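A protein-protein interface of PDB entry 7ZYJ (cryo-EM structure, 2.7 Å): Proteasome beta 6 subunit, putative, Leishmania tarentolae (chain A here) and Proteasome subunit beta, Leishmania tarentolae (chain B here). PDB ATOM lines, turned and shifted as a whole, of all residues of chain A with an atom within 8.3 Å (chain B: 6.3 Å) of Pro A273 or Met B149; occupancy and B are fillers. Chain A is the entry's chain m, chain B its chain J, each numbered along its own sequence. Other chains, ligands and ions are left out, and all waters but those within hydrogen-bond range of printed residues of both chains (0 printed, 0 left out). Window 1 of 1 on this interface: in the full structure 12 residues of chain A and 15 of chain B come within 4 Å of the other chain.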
ATOM      1  N   TYR A 261     -40.082  20.513   0.708  1.00  0.00           N
ATOM      2  CA  TYR A 261     -39.853  21.446  -0.382  1.00  0.00           C
ATOM      3  C   TYR A 261     -39.570  20.648  -1.646  1.00  0.00           C
ATOM      4  O   TYR A 261     -39.577  19.413  -1.644  1.00  0.00           O
ATOM      5  CB  TYR A 261     -38.714  22.425  -0.067  1.00  0.00           C
ATOM      6  CG  TYR A 261     -37.446  21.781   0.443  1.00  0.00           C
ATOM      7  CD1 TYR A 261     -36.453  21.371  -0.435  1.00  0.00           C
ATOM      8  CD2 TYR A 261     -37.233  21.600   1.802  1.00  0.00           C
ATOM      9  CE1 TYR A 261     -35.290  20.789   0.024  1.00  0.00           C
ATOM     10  CE2 TYR A 261     -36.072  21.018   2.272  1.00  0.00           C
ATOM     11  CZ  TYR A 261     -35.105  20.615   1.377  1.00  0.00           C
ATOM     12  OH  TYR A 261     -33.947  20.034   1.839  1.00  0.00           O
ATOM     13  N   THR A 263     -38.141  21.435  -6.118  1.00  0.00           N
ATOM     14  CA  THR A 263     -38.040  22.253  -7.317  1.00  0.00           C
ATOM     15  C   THR A 263     -38.051  21.355  -8.543  1.00  0.00           C
ATOM     16  O   THR A 263     -37.391  20.312  -8.566  1.00  0.00           O
ATOM     17  CB  THR A 263     -36.770  23.104  -7.310  1.00  0.00           C
ATOM     18  OG1 THR A 263     -35.623  22.247  -7.281  1.00  0.00           O
ATOM     19  CG2 THR A 263     -36.747  24.000  -6.088  1.00  0.00           C
ATOM     20  N   ALA A 267     -34.389  24.868 -14.010  1.00  0.00           N
ATOM     21  CA  ALA A 267     -33.481  25.449 -13.027  1.00  0.00           C
ATOM     22  C   ALA A 267     -33.514  24.713 -11.692  1.00  0.00           C
ATOM     23  O   ALA A 267     -33.098  25.269 -10.670  1.00  0.00           O
ATOM     24  CB  ALA A 267     -33.803  26.928 -12.825  1.00  0.00           C
ATOM     25  N   ALA A 268     -34.005  23.472 -11.679  1.00  0.00           N
ATOM     26  CA  ALA A 268     -34.098  22.721 -10.430  1.00  0.00           C
ATOM     27  C   ALA A 268     -32.720  22.465  -9.833  1.00  0.00           C
ATOM     28  O   ALA A 268     -32.524  22.595  -8.619  1.00  0.00           O
ATOM     29  CB  ALA A 268     -34.837  21.405 -10.667  1.00  0.00           C
ATOM     30  N   SER A 269     -31.749  22.099 -10.672  1.00  0.00           N
ATOM     31  CA  SER A 269     -30.402  21.808 -10.193  1.00  0.00           C
ATOM     32  C   SER A 269     -29.681  23.040  -9.667  1.00  0.00           C
ATOM     33  O   SER A 269     -28.664  22.894  -8.981  1.00  0.00           O
ATOM     34  CB  SER A 269     -29.578  21.169 -11.311  1.00  0.00           C
ATOM     35  OG  SER A 269     -28.261  20.883 -10.874  1.00  0.00           O
ATOM     36  N   PHE A 270     -30.171  24.241  -9.970  1.00  0.00           N
ATOM     37  CA  PHE A 270     -29.529  25.467  -9.515  1.00  0.00           C
ATOM     38  C   PHE A 270     -30.051  25.932  -8.163  1.00  0.00           C
ATOM     39  O   PHE A 270     -29.313  26.565  -7.400  1.00  0.00           O
ATOM     40  CB  PHE A 270     -29.724  26.578 -10.549  1.00  0.00           C
ATOM     41  CG  PHE A 270     -28.809  26.472 -11.732  1.00  0.00           C
ATOM     42  CD1 PHE A 270     -27.551  27.048 -11.703  1.00  0.00           C
ATOM     43  CD2 PHE A 270     -29.205  25.793 -12.871  1.00  0.00           C
ATOM     44  CE1 PHE A 270     -26.706  26.951 -12.790  1.00  0.00           C
ATOM     45  CE2 PHE A 270     -28.364  25.693 -13.961  1.00  0.00           C
ATOM     46  CZ  PHE A 270     -27.112  26.272 -13.920  1.00  0.00           C
ATOM     47  N   VAL A 271     -31.310  25.632  -7.848  1.00  0.00           N
ATOM     48  CA  VAL A 271     -31.939  26.147  -6.646  1.00  0.00           C
ATOM     49  C   VAL A 271     -32.174  25.070  -5.591  1.00  0.00           C
ATOM     50  O   VAL A 271     -32.225  25.397  -4.400  1.00  0.00           O
ATOM     51  CB  VAL A 271     -33.258  26.868  -6.993  1.00  0.00           C
ATOM     52  CG1 VAL A 271     -32.982  28.054  -7.891  1.00  0.00           C
ATOM     53  CG2 VAL A 271     -34.216  25.915  -7.675  1.00  0.00           C
ATOM     54  N   GLU A 272     -32.326  23.806  -5.984  1.00  0.00           N
ATOM     55  CA  GLU A 272     -32.532  22.751  -4.995  1.00  0.00           C
ATOM     56  C   GLU A 272     -31.369  22.602  -4.018  1.00  0.00           C
ATOM     57  O   GLU A 272     -31.636  22.488  -2.807  1.00  0.00           O
ATOM     58  CB  GLU A 272     -32.827  21.425  -5.708  1.00  0.00           C
ATOM     59  CG  GLU A 272     -33.434  20.363  -4.808  1.00  0.00           C
ATOM     60  CD  GLU A 272     -34.199  19.308  -5.582  1.00  0.00           C
ATOM     61  OE1 GLU A 272     -35.221  18.814  -5.064  1.00  0.00           O
ATOM     62  OE2 GLU A 272     -33.777  18.974  -6.709  1.00  0.00           O
ATOM     63  N   PRO A 273     -30.098  22.577  -4.437  1.00  0.00           N
ATOM     64  CA  PRO A 273     -29.017  22.541  -3.439  1.00  0.00           C
ATOM     65  C   PRO A 273     -29.004  23.751  -2.525  1.00  0.00           C
ATOM     66  O   PRO A 273     -28.611  23.630  -1.359  1.00  0.00           O
ATOM     67  CB  PRO A 273     -27.744  22.468  -4.296  1.00  0.00           C
ATOM     68  CG  PRO A 273     -28.196  21.954  -5.609  1.00  0.00           C
ATOM     69  CD  PRO A 273     -29.562  22.513  -5.809  1.00  0.00           C
ATOM     70  N   LEU A 274     -29.413  24.920  -3.023  1.00  0.00           N
ATOM     71  CA  LEU A 274     -29.471  26.104  -2.175  1.00  0.00           C
ATOM     72  C   LEU A 274     -30.541  25.961  -1.101  1.00  0.00           C
ATOM     73  O   LEU A 274     -30.316  26.328   0.059  1.00  0.00           O
ATOM     74  CB  LEU A 274     -29.721  27.347  -3.026  1.00  0.00           C
ATOM     75  CG  LEU A 274     -30.050  28.620  -2.249  1.00  0.00           C
ATOM     76  CD1 LEU A 274     -28.812  29.133  -1.539  1.00  0.00           C
ATOM     77  CD2 LEU A 274     -30.620  29.679  -3.177  1.00  0.00           C
ATOM     78  N   LEU A 275     -31.709  25.430  -1.467  1.00  0.00           N
ATOM     79  CA  LEU A 275     -32.733  25.150  -0.468  1.00  0.00           C
ATOM     80  C   LEU A 275     -32.260  24.087   0.515  1.00  0.00           C
ATOM     81  O   LEU A 275     -32.598  24.133   1.702  1.00  0.00           O
ATOM     82  CB  LEU A 275     -34.030  24.714  -1.147  1.00  0.00           C
ATOM     83  CG  LEU A 275     -34.697  25.739  -2.065  1.00  0.00           C
ATOM     84  CD1 LEU A 275     -35.914  25.135  -2.739  1.00  0.00           C
ATOM     85  CD2 LEU A 275     -35.074  26.988  -1.291  1.00  0.00           C
ATOM     86  N   ASP A 276     -31.476  23.119   0.033  1.00  0.00           N
ATOM     87  CA  ASP A 276     -30.927  22.101   0.922  1.00  0.00           C
ATOM     88  C   ASP A 276     -30.018  22.711   1.982  1.00  0.00           C
ATOM     89  O   ASP A 276     -30.081  22.320   3.152  1.00  0.00           O
ATOM     90  CB  ASP A 276     -30.159  21.055   0.114  1.00  0.00           C
ATOM     91  CG  ASP A 276     -31.073  20.120  -0.647  1.00  0.00           C
ATOM     92  OD1 ASP A 276     -32.269  20.044  -0.300  1.00  0.00           O
ATOM     93  OD2 ASP A 276     -30.595  19.458  -1.590  1.00  0.00           O
ATOM     94  N   CYS A 277     -29.171  23.664   1.594  1.00  0.00           N
ATOM     95  CA  CYS A 277     -28.217  24.246   2.532  1.00  0.00           C
ATOM     96  C   CYS A 277     -28.885  25.159   3.552  1.00  0.00           C
ATOM     97  O   CYS A 277     -28.515  25.136   4.731  1.00  0.00           O
ATOM     98  CB  CYS A 277     -27.139  25.017   1.767  1.00  0.00           C
ATOM     99  SG  CYS A 277     -26.133  26.118   2.787  1.00  0.00           S
ATOM    100  N   LEU A 278     -29.863  25.960   3.130  1.00  0.00           N
ATOM    101  CA  LEU A 278     -30.470  26.948   4.013  1.00  0.00           C
ATOM    102  C   LEU A 278     -31.575  26.382   4.893  1.00  0.00           C
ATOM    103  O   LEU A 278     -31.891  26.985   5.925  1.00  0.00           O
ATOM    104  CB  LEU A 278     -31.034  28.113   3.196  1.00  0.00           C
ATOM    105  CG  LEU A 278     -30.071  28.876   2.287  1.00  0.00           C
ATOM    106  CD1 LEU A 278     -30.840  29.858   1.424  1.00  0.00           C
ATOM    107  CD2 LEU A 278     -29.013  29.593   3.108  1.00  0.00           C
ATOM    108  N   ILE A 279     -32.168  25.254   4.522  1.00  0.00           N
ATOM    109  CA  ILE A 279     -33.254  24.652   5.289  1.00  0.00           C
ATOM    110  C   ILE A 279     -32.751  23.525   6.181  1.00  0.00           C
ATOM    111  O   ILE A 279     -33.021  23.507   7.381  1.00  0.00           O
ATOM    112  CB  ILE A 279     -34.373  24.163   4.341  1.00  0.00           C
ATOM    113  CG1 ILE A 279     -35.004  25.349   3.610  1.00  0.00           C
ATOM    114  CG2 ILE A 279     -35.424  23.388   5.114  1.00  0.00           C
ATOM    115  CD1 ILE A 279     -36.041  24.955   2.583  1.00  0.00           C
ATOM    116  N   ASN A 280     -32.011  22.573   5.610  1.00  0.00           N
ATOM    117  CA  ASN A 280     -31.483  21.470   6.403  1.00  0.00           C
ATOM    118  C   ASN A 280     -30.320  21.896   7.287  1.00  0.00           C
ATOM    119  O   ASN A 280     -30.107  21.286   8.340  1.00  0.00           O
ATOM    120  CB  ASN A 280     -31.055  20.319   5.492  1.00  0.00           C
ATOM    121  CG  ASN A 280     -32.217  19.719   4.729  1.00  0.00           C
ATOM    122  OD1 ASN A 280     -32.280  19.804   3.503  1.00  0.00           O
ATOM    123  ND2 ASN A 280     -33.146  19.106   5.452  1.00  0.00           N
ATOM    124  N   MET A 284     -22.986  22.472   9.262  1.00  0.00           N
ATOM    125  CA  MET A 284     -22.941  23.760   9.940  1.00  0.00           C
ATOM    126  C   MET A 284     -22.783  23.513  11.431  1.00  0.00           C
ATOM    127  O   MET A 284     -23.678  22.947  12.065  1.00  0.00           O
ATOM    128  CB  MET A 284     -24.207  24.573   9.659  1.00  0.00           C
ATOM    129  CG  MET A 284     -24.089  25.512   8.472  1.00  0.00           C
ATOM    130  SD  MET A 284     -25.693  25.913   7.757  1.00  0.00           S
ATOM    131  CE  MET A 284     -25.216  27.055   6.466  1.00  0.00           C
ATOM    132  N   GLY A 307     -31.544  34.106  -8.493  1.00  0.00           N
ATOM    133  CA  GLY A 307     -30.299  33.456  -8.857  1.00  0.00           C
ATOM    134  C   GLY A 307     -30.437  32.525 -10.043  1.00  0.00           C
ATOM    135  O   GLY A 307     -29.541  32.456 -10.888  1.00  0.00           O
ATOM    136  N   ARG A 311     -28.612  32.574 -14.453  1.00  0.00           N
ATOM    137  CA  ARG A 311     -27.735  31.524 -14.959  1.00  0.00           C
ATOM    138  C   ARG A 311     -28.422  30.528 -15.878  1.00  0.00           C
ATOM    139  O   ARG A 311     -27.725  29.857 -16.649  1.00  0.00           O
ATOM    140  CB  ARG A 311     -27.088  30.757 -13.796  1.00  0.00           C
ATOM    141  CG  ARG A 311     -26.121  31.592 -12.972  1.00  0.00           C
ATOM    142  CD  ARG A 311     -24.751  31.652 -13.625  1.00  0.00           C
ATOM    143  NE  ARG A 311     -23.897  32.657 -13.006  1.00  0.00           N
ATOM    144  CZ  ARG A 311     -22.698  33.000 -13.456  1.00  0.00           C
ATOM    145  NH1 ARG A 311     -22.174  32.432 -14.529  1.00  0.00           N
ATOM    146  NH2 ARG A 311     -22.007  33.937 -12.813  1.00  0.00           N
ATOM    147  N   MET B  14     -12.833  30.596  -6.189  1.00  0.00           N
ATOM    148  CA  MET B  14     -13.613  31.744  -5.760  1.00  0.00           C
ATOM    149  C   MET B  14     -12.660  32.867  -5.380  1.00  0.00           C
ATOM    150  O   MET B  14     -11.587  32.624  -4.823  1.00  0.00           O
ATOM    151  CB  MET B  14     -14.515  31.376  -4.578  1.00  0.00           C
ATOM    152  CG  MET B  14     -15.554  32.410  -4.226  1.00  0.00           C
ATOM    153  SD  MET B  14     -16.615  31.854  -2.882  1.00  0.00           S
ATOM    154  CE  MET B  14     -17.590  30.612  -3.721  1.00  0.00           C
ATOM    155  N   GLU B 144     -23.383  22.624 -12.237  1.00  0.00           N
ATOM    156  CA  GLU B 144     -24.609  23.413 -12.141  1.00  0.00           C
ATOM    157  C   GLU B 144     -24.915  23.785 -10.695  1.00  0.00           C
ATOM    158  O   GLU B 144     -25.238  24.942 -10.390  1.00  0.00           O
ATOM    159  CB  GLU B 144     -25.779  22.646 -12.758  1.00  0.00           C
ATOM    160  CG  GLU B 144     -25.576  22.229 -14.209  1.00  0.00           C
ATOM    161  CD  GLU B 144     -24.752  20.963 -14.356  1.00  0.00           C
ATOM    162  OE1 GLU B 144     -24.252  20.450 -13.333  1.00  0.00           O
ATOM    163  OE2 GLU B 144     -24.606  20.479 -15.499  1.00  0.00           O
ATOM    164  N   SER B 145     -24.824  22.812  -9.788  1.00  0.00           N
ATOM    165  CA  SER B 145     -25.073  23.089  -8.378  1.00  0.00           C
ATOM    166  C   SER B 145     -24.030  24.039  -7.805  1.00  0.00           C
ATOM    167  O   SER B 145     -24.364  24.914  -6.997  1.00  0.00           O
ATOM    168  CB  SER B 145     -25.102  21.783  -7.587  1.00  0.00           C
ATOM    169  OG  SER B 145     -26.175  20.960  -8.007  1.00  0.00           O
ATOM    170  N   LEU B 146     -22.767  23.879  -8.207  1.00  0.00           N
ATOM    171  CA  LEU B 146     -21.726  24.802  -7.772  1.00  0.00           C
ATOM    172  C   LEU B 146     -22.020  26.217  -8.255  1.00  0.00           C
ATOM    173  O   LEU B 146     -21.868  27.186  -7.501  1.00  0.00           O
ATOM    174  CB  LEU B 146     -20.364  24.334  -8.282  1.00  0.00           C
ATOM    175  CG  LEU B 146     -19.638  23.276  -7.449  1.00  0.00           C
ATOM    176  CD1 LEU B 146     -18.470  22.691  -8.227  1.00  0.00           C
ATOM    177  CD2 LEU B 146     -19.172  23.861  -6.126  1.00  0.00           C
ATOM    178  N   HIS B 147     -22.444  26.352  -9.514  1.00  0.00           N
ATOM    179  CA  HIS B 147     -22.802  27.663 -10.042  1.00  0.00           C
ATOM    180  C   HIS B 147     -23.941  28.280  -9.246  1.00  0.00           C
ATOM    181  O   HIS B 147     -23.887  29.459  -8.886  1.00  0.00           O
ATOM    182  CB  HIS B 147     -23.194  27.550 -11.516  1.00  0.00           C
ATOM    183  CG  HIS B 147     -22.047  27.706 -12.464  1.00  0.00           C
ATOM    184  ND1 HIS B 147     -21.288  28.854 -12.534  1.00  0.00           N
ATOM    185  CD2 HIS B 147     -21.539  26.863 -13.394  1.00  0.00           C
ATOM    186  CE1 HIS B 147     -20.356  28.707 -13.458  1.00  0.00           C
ATOM    187  NE2 HIS B 147     -20.487  27.508 -13.995  1.00  0.00           N
ATOM    188  N   GLY B 148     -24.978  27.492  -8.956  1.00  0.00           N
ATOM    189  CA  GLY B 148     -26.097  28.018  -8.189  1.00  0.00           C
ATOM    190  C   GLY B 148     -25.692  28.468  -6.798  1.00  0.00           C
ATOM    191  O   GLY B 148     -26.052  29.564  -6.359  1.00  0.00           O
ATOM    192  N   MET B 149     -24.921  27.636  -6.094  1.00  0.00           N
ATOM    193  CA  MET B 149     -24.505  27.983  -4.739  1.00  0.00           C
ATOM    194  C   MET B 149     -23.607  29.214  -4.727  1.00  0.00           C
ATOM    195  O   MET B 149     -23.767  30.096  -3.875  1.00  0.00           O
ATOM    196  CB  MET B 149     -23.793  26.797  -4.090  1.00  0.00           C
ATOM    197  CG  MET B 149     -24.684  25.596  -3.836  1.00  0.00           C
ATOM    198  SD  MET B 149     -25.998  25.934  -2.651  1.00  0.00           S
ATOM    199  CE  MET B 149     -25.084  26.705  -1.321  1.00  0.00           C
ATOM    200  N   CYS B 150     -22.656  29.293  -5.663  1.00  0.00           N
ATOM    201  CA  CYS B 150     -21.773  30.453  -5.719  1.00  0.00           C
ATOM    202  C   CYS B 150     -22.543  31.717  -6.080  1.00  0.00           C
ATOM    203  O   CYS B 150     -22.294  32.783  -5.507  1.00  0.00           O
ATOM    204  CB  CYS B 150     -20.643  30.205  -6.715  1.00  0.00           C
ATOM    205  SG  CYS B 150     -19.526  28.863  -6.259  1.00  0.00           S
ATOM    206  N   GLU B 151     -23.480  31.621  -7.025  1.00  0.00           N
ATOM    207  CA  GLU B 151     -24.306  32.771  -7.368  1.00  0.00           C
ATOM    208  C   GLU B 151     -25.135  33.233  -6.178  1.00  0.00           C
ATOM    209  O   GLU B 151     -25.340  34.438  -5.995  1.00  0.00           O
ATOM    210  CB  GLU B 151     -25.214  32.424  -8.548  1.00  0.00           C
ATOM    211  CG  GLU B 151     -26.165  33.534  -8.960  1.00  0.00           C
ATOM    212  CD  GLU B 151     -25.448  34.731  -9.552  1.00  0.00           C
ATOM    213  OE1 GLU B 151     -24.394  34.536 -10.193  1.00  0.00           O
ATOM    214  OE2 GLU B 151     -25.937  35.866  -9.373  1.00  0.00           O
ATOM    215  N   ALA B 152     -25.608  32.297  -5.359  1.00  0.00           N
ATOM    216  CA  ALA B 152     -26.442  32.641  -4.216  1.00  0.00           C
ATOM    217  C   ALA B 152     -25.659  33.117  -2.999  1.00  0.00           C
ATOM    218  O   ALA B 152     -26.229  33.811  -2.152  1.00  0.00           O
ATOM    219  CB  ALA B 152     -27.302  31.439  -3.814  1.00  0.00           C
ATOM    220  N   LEU B 153     -24.375  32.774  -2.883  1.00  0.00           N
ATOM    221  CA  LEU B 153     -23.636  33.061  -1.657  1.00  0.00           C
ATOM    222  C   LEU B 153     -22.521  34.087  -1.817  1.00  0.00           C
ATOM    223  O   LEU B 153     -22.150  34.728  -0.829  1.00  0.00           O
ATOM    224  CB  LEU B 153     -23.034  31.773  -1.089  1.00  0.00           C
ATOM    225  CG  LEU B 153     -24.007  30.702  -0.596  1.00  0.00           C
ATOM    226  CD1 LEU B 153     -23.243  29.560   0.050  1.00  0.00           C
ATOM    227  CD2 LEU B 153     -25.013  31.297   0.373  1.00  0.00           C
ATOM    228  N   TRP B 154     -21.973  34.261  -3.015  1.00  0.00           N
ATOM    229  CA  TRP B 154     -20.774  35.073  -3.185  1.00  0.00           C
ATOM    230  C   TRP B 154     -21.087  36.564  -3.166  1.00  0.00           C
ATOM    231  O   TRP B 154     -22.108  37.011  -3.695  1.00  0.00           O
ATOM    232  CB  TRP B 154     -20.067  34.707  -4.490  1.00  0.00           C
ATOM    233  CG  TRP B 154     -18.802  35.472  -4.724  1.00  0.00           C
ATOM    234  CD1 TRP B 154     -17.547  35.116  -4.335  1.00  0.00           C
ATOM    235  CD2 TRP B 154     -18.669  36.716  -5.422  1.00  0.00           C
ATOM    236  NE1 TRP B 154     -16.640  36.066  -4.735  1.00  0.00           N
ATOM    237  CE2 TRP B 154     -17.304  37.058  -5.406  1.00  0.00           C
ATOM    238  CE3 TRP B 154     -19.573  37.575  -6.054  1.00  0.00           C
ATOM    239  CZ2 TRP B 154     -16.821  38.222  -5.997  1.00  0.00           C
ATOM    240  CZ3 TRP B 154     -19.091  38.729  -6.639  1.00  0.00           C
ATOM    241  CH2 TRP B 154     -17.727  39.041  -6.610  1.00  0.00           C
ATOM    242  N   ILE B 166     -17.680  30.231   2.566  1.00  0.00           N
ATOM    243  CA  ILE B 166     -18.613  30.217   1.442  1.00  0.00           C
ATOM    244  C   ILE B 166     -18.255  29.101   0.469  1.00  0.00           C
ATOM    245  O   ILE B 166     -19.125  28.349   0.010  1.00  0.00           O
ATOM    246  CB  ILE B 166     -18.635  31.588   0.744  1.00  0.00           C
ATOM    247  CG1 ILE B 166     -19.215  32.653   1.674  1.00  0.00           C
ATOM    248  CG2 ILE B 166     -19.431  31.519  -0.549  1.00  0.00           C
ATOM    249  CD1 ILE B 166     -20.669  32.442   2.013  1.00  0.00           C
ATOM    250  N   GLN B 169     -19.102  25.611   2.011  1.00  0.00           N
ATOM    251  CA  GLN B 169     -20.538  25.355   2.015  1.00  0.00           C
ATOM    252  C   GLN B 169     -21.044  25.061   0.610  1.00  0.00           C
ATOM    253  O   GLN B 169     -21.807  24.109   0.398  1.00  0.00           O
ATOM    254  CB  GLN B 169     -21.282  26.546   2.618  1.00  0.00           C
ATOM    255  CG  GLN B 169     -21.409  26.489   4.129  1.00  0.00           C
ATOM    256  CD  GLN B 169     -22.012  25.186   4.610  1.00  0.00           C
ATOM    257  OE1 GLN B 169     -21.348  24.390   5.272  1.00  0.00           O
ATOM    258  NE2 GLN B 169     -23.277  24.962   4.278  1.00  0.00           N
ATOM    259  N   ALA B 170     -20.619  25.865  -0.369  1.00  0.00           N
ATOM    260  CA  ALA B 170     -21.054  25.654  -1.745  1.00  0.00           C
ATOM    261  C   ALA B 170     -20.602  24.294  -2.259  1.00  0.00           C
ATOM    262  O   ALA B 170     -21.381  23.562  -2.880  1.00  0.00           O
ATOM    263  CB  ALA B 170     -20.521  26.774  -2.636  1.00  0.00           C
ATOM    264  N   MET B 171     -19.345  23.933  -1.993  1.00  0.00           N
ATOM    265  CA  MET B 171     -18.814  22.662  -2.470  1.00  0.00           C
ATOM    266  C   MET B 171     -19.561  21.487  -1.855  1.00  0.00           C
ATOM    267  O   MET B 171     -19.941  20.547  -2.564  1.00  0.00           O
ATOM    268  CB  MET B 171     -17.324  22.574  -2.147  1.00  0.00           C
ATOM    269  CG  MET B 171     -16.598  21.413  -2.797  1.00  0.00           C
ATOM    270  SD  MET B 171     -16.177  21.764  -4.512  1.00  0.00           S
ATOM    271  CE  MET B 171     -17.039  20.444  -5.348  1.00  0.00           C
ATOM    272  N   SER B 173     -22.610  21.425  -0.474  1.00  0.00           N
ATOM    273  CA  SER B 173     -23.996  21.377  -0.920  1.00  0.00           C
ATOM    274  C   SER B 173     -24.108  20.925  -2.369  1.00  0.00           C
ATOM    275  O   SER B 173     -25.090  20.270  -2.736  1.00  0.00           O
ATOM    276  CB  SER B 173     -24.651  22.744  -0.731  1.00  0.00           C
ATOM    277  OG  SER B 173     -23.873  23.758  -1.336  1.00  0.00           O
ATOM    278  N   ALA B 174     -23.125  21.261  -3.207  1.00  0.00           N
ATOM    279  CA  ALA B 174     -23.144  20.791  -4.586  1.00  0.00           C
ATOM    280  C   ALA B 174     -22.828  19.303  -4.673  1.00  0.00           C
ATOM    281  O   ALA B 174     -23.418  18.589  -5.491  1.00  0.00           O
ATOM    282  CB  ALA B 174     -22.157  21.595  -5.428  1.00  0.00           C
ATOM    283  N   ARG B 177     -25.824  16.804  -3.913  1.00  0.00           N
ATOM    284  CA  ARG B 177     -26.757  16.535  -4.998  1.00  0.00           C
ATOM    285  C   ARG B 177     -26.112  15.800  -6.166  1.00  0.00           C
ATOM    286  O   ARG B 177     -26.790  15.532  -7.162  1.00  0.00           O
ATOM    287  CB  ARG B 177     -27.379  17.844  -5.490  1.00  0.00           C
ATOM    288  CG  ARG B 177     -28.466  18.392  -4.583  1.00  0.00           C
ATOM    289  CD  ARG B 177     -29.730  17.555  -4.671  1.00  0.00           C
ATOM    290  NE  ARG B 177     -30.663  17.863  -3.594  1.00  0.00           N
ATOM    291  CZ  ARG B 177     -31.827  17.255  -3.416  1.00  0.00           C
ATOM    292  NH1 ARG B 177     -32.239  16.297  -4.230  1.00  0.00           N
ATOM    293  NH2 ARG B 177     -32.598  17.616  -2.393  1.00  0.00           N
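OE1 of Glu B151 lies within salt-bridge range of NE of Arg A311, 3.4 Å away. The guanidinium group (NE) of Arg B177 is in salt-bridge range of the side-chain carboxylate (OD2) of Asp A276. NH2 of Arg B177 lies within salt-bridge range of OE1 of Glu A272, 3.9 Å away. NE2 of Gln B169 lies within hydrogen-bond range of SG of Cys A277 (3.4 Å). SD of Met B149 lies close to N of Leu A274, at 3.6 Å. The side-chain sulfur (SD) of Met B149 lies close to the backbone carbonyl oxygen (O) of Pro A273 (3.7 Å). The side-chain hydroxyl (OG) of Ser B145 is in hydrogen-bond range of the backbone carbonyl oxygen (O) of Ser A269 (3.3 Å).
The side-chain sulfur (SD) of Met B149 sits close to the side-chain hydroxyl (OG) of Ser B173 (3.3 Å). The backbone carbonyl oxygen (O) of Gln B169 lies within hydrogen-bond range of the side-chain hydroxyl (OG) of Ser B173 (2.7 Å). OD1 of Asp A276 is in hydrogen-bond range of OH of Tyr A261, 2.7 Å away. OD1 of Asn A280 sits close to O of Asp A276. The backbone carbonyl oxygen (O) of Ala B170 sits at hydrogen-bond distance from the side-chain hydroxyl (OG) of Ser B173 (2.9 Å).
OG of Ser A269 touches CB of Glu B144 (3.6 Å). CD1 of Phe A270 touches O of Glu B144 (3.4 Å). His B147 touches Phe A270 (CB to CE1, 3.8 Å). Gly B148 touches Phe A270. OG of Ser B145 touches CG of Pro A273, at 3.3 Å. Pro A273 touches Ser B173 (CB to O, 3.8 Å). Pro A273 touches Arg B177. Leu A274 touches Ala B152 (CD1 to CB, 3.6 Å). Met A284 touches Gln B169.
Pro A273 touches just these residues of chain B: Ser B145, Met B149, Ser B173 and Arg B177. Of the printed residues of chain B, Cys A277 touches Gln B169 (3.4 Å). Of the printed residues of chain A, His B147 touches Phe A270 (3.8 Å). Printed residues of chain A within 4 Å of Gly B148: Phe A270 (3.6 Å). Met B149 touches just these residues of chain A: Pro A273 (3.7 Å) and Leu A274 (3.5 Å). The nearest residue of chain A that does not touch Met B149 is Cys A277 (4.1 Å). The nearest printed residue of chain B that does not touch Leu A274 is Leu B153 (4.8 Å).
Of the 19 printed residues of chain A, 9 touch a printed residue of chain B. Among the printed residues, 16 pairs touch across the chains.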
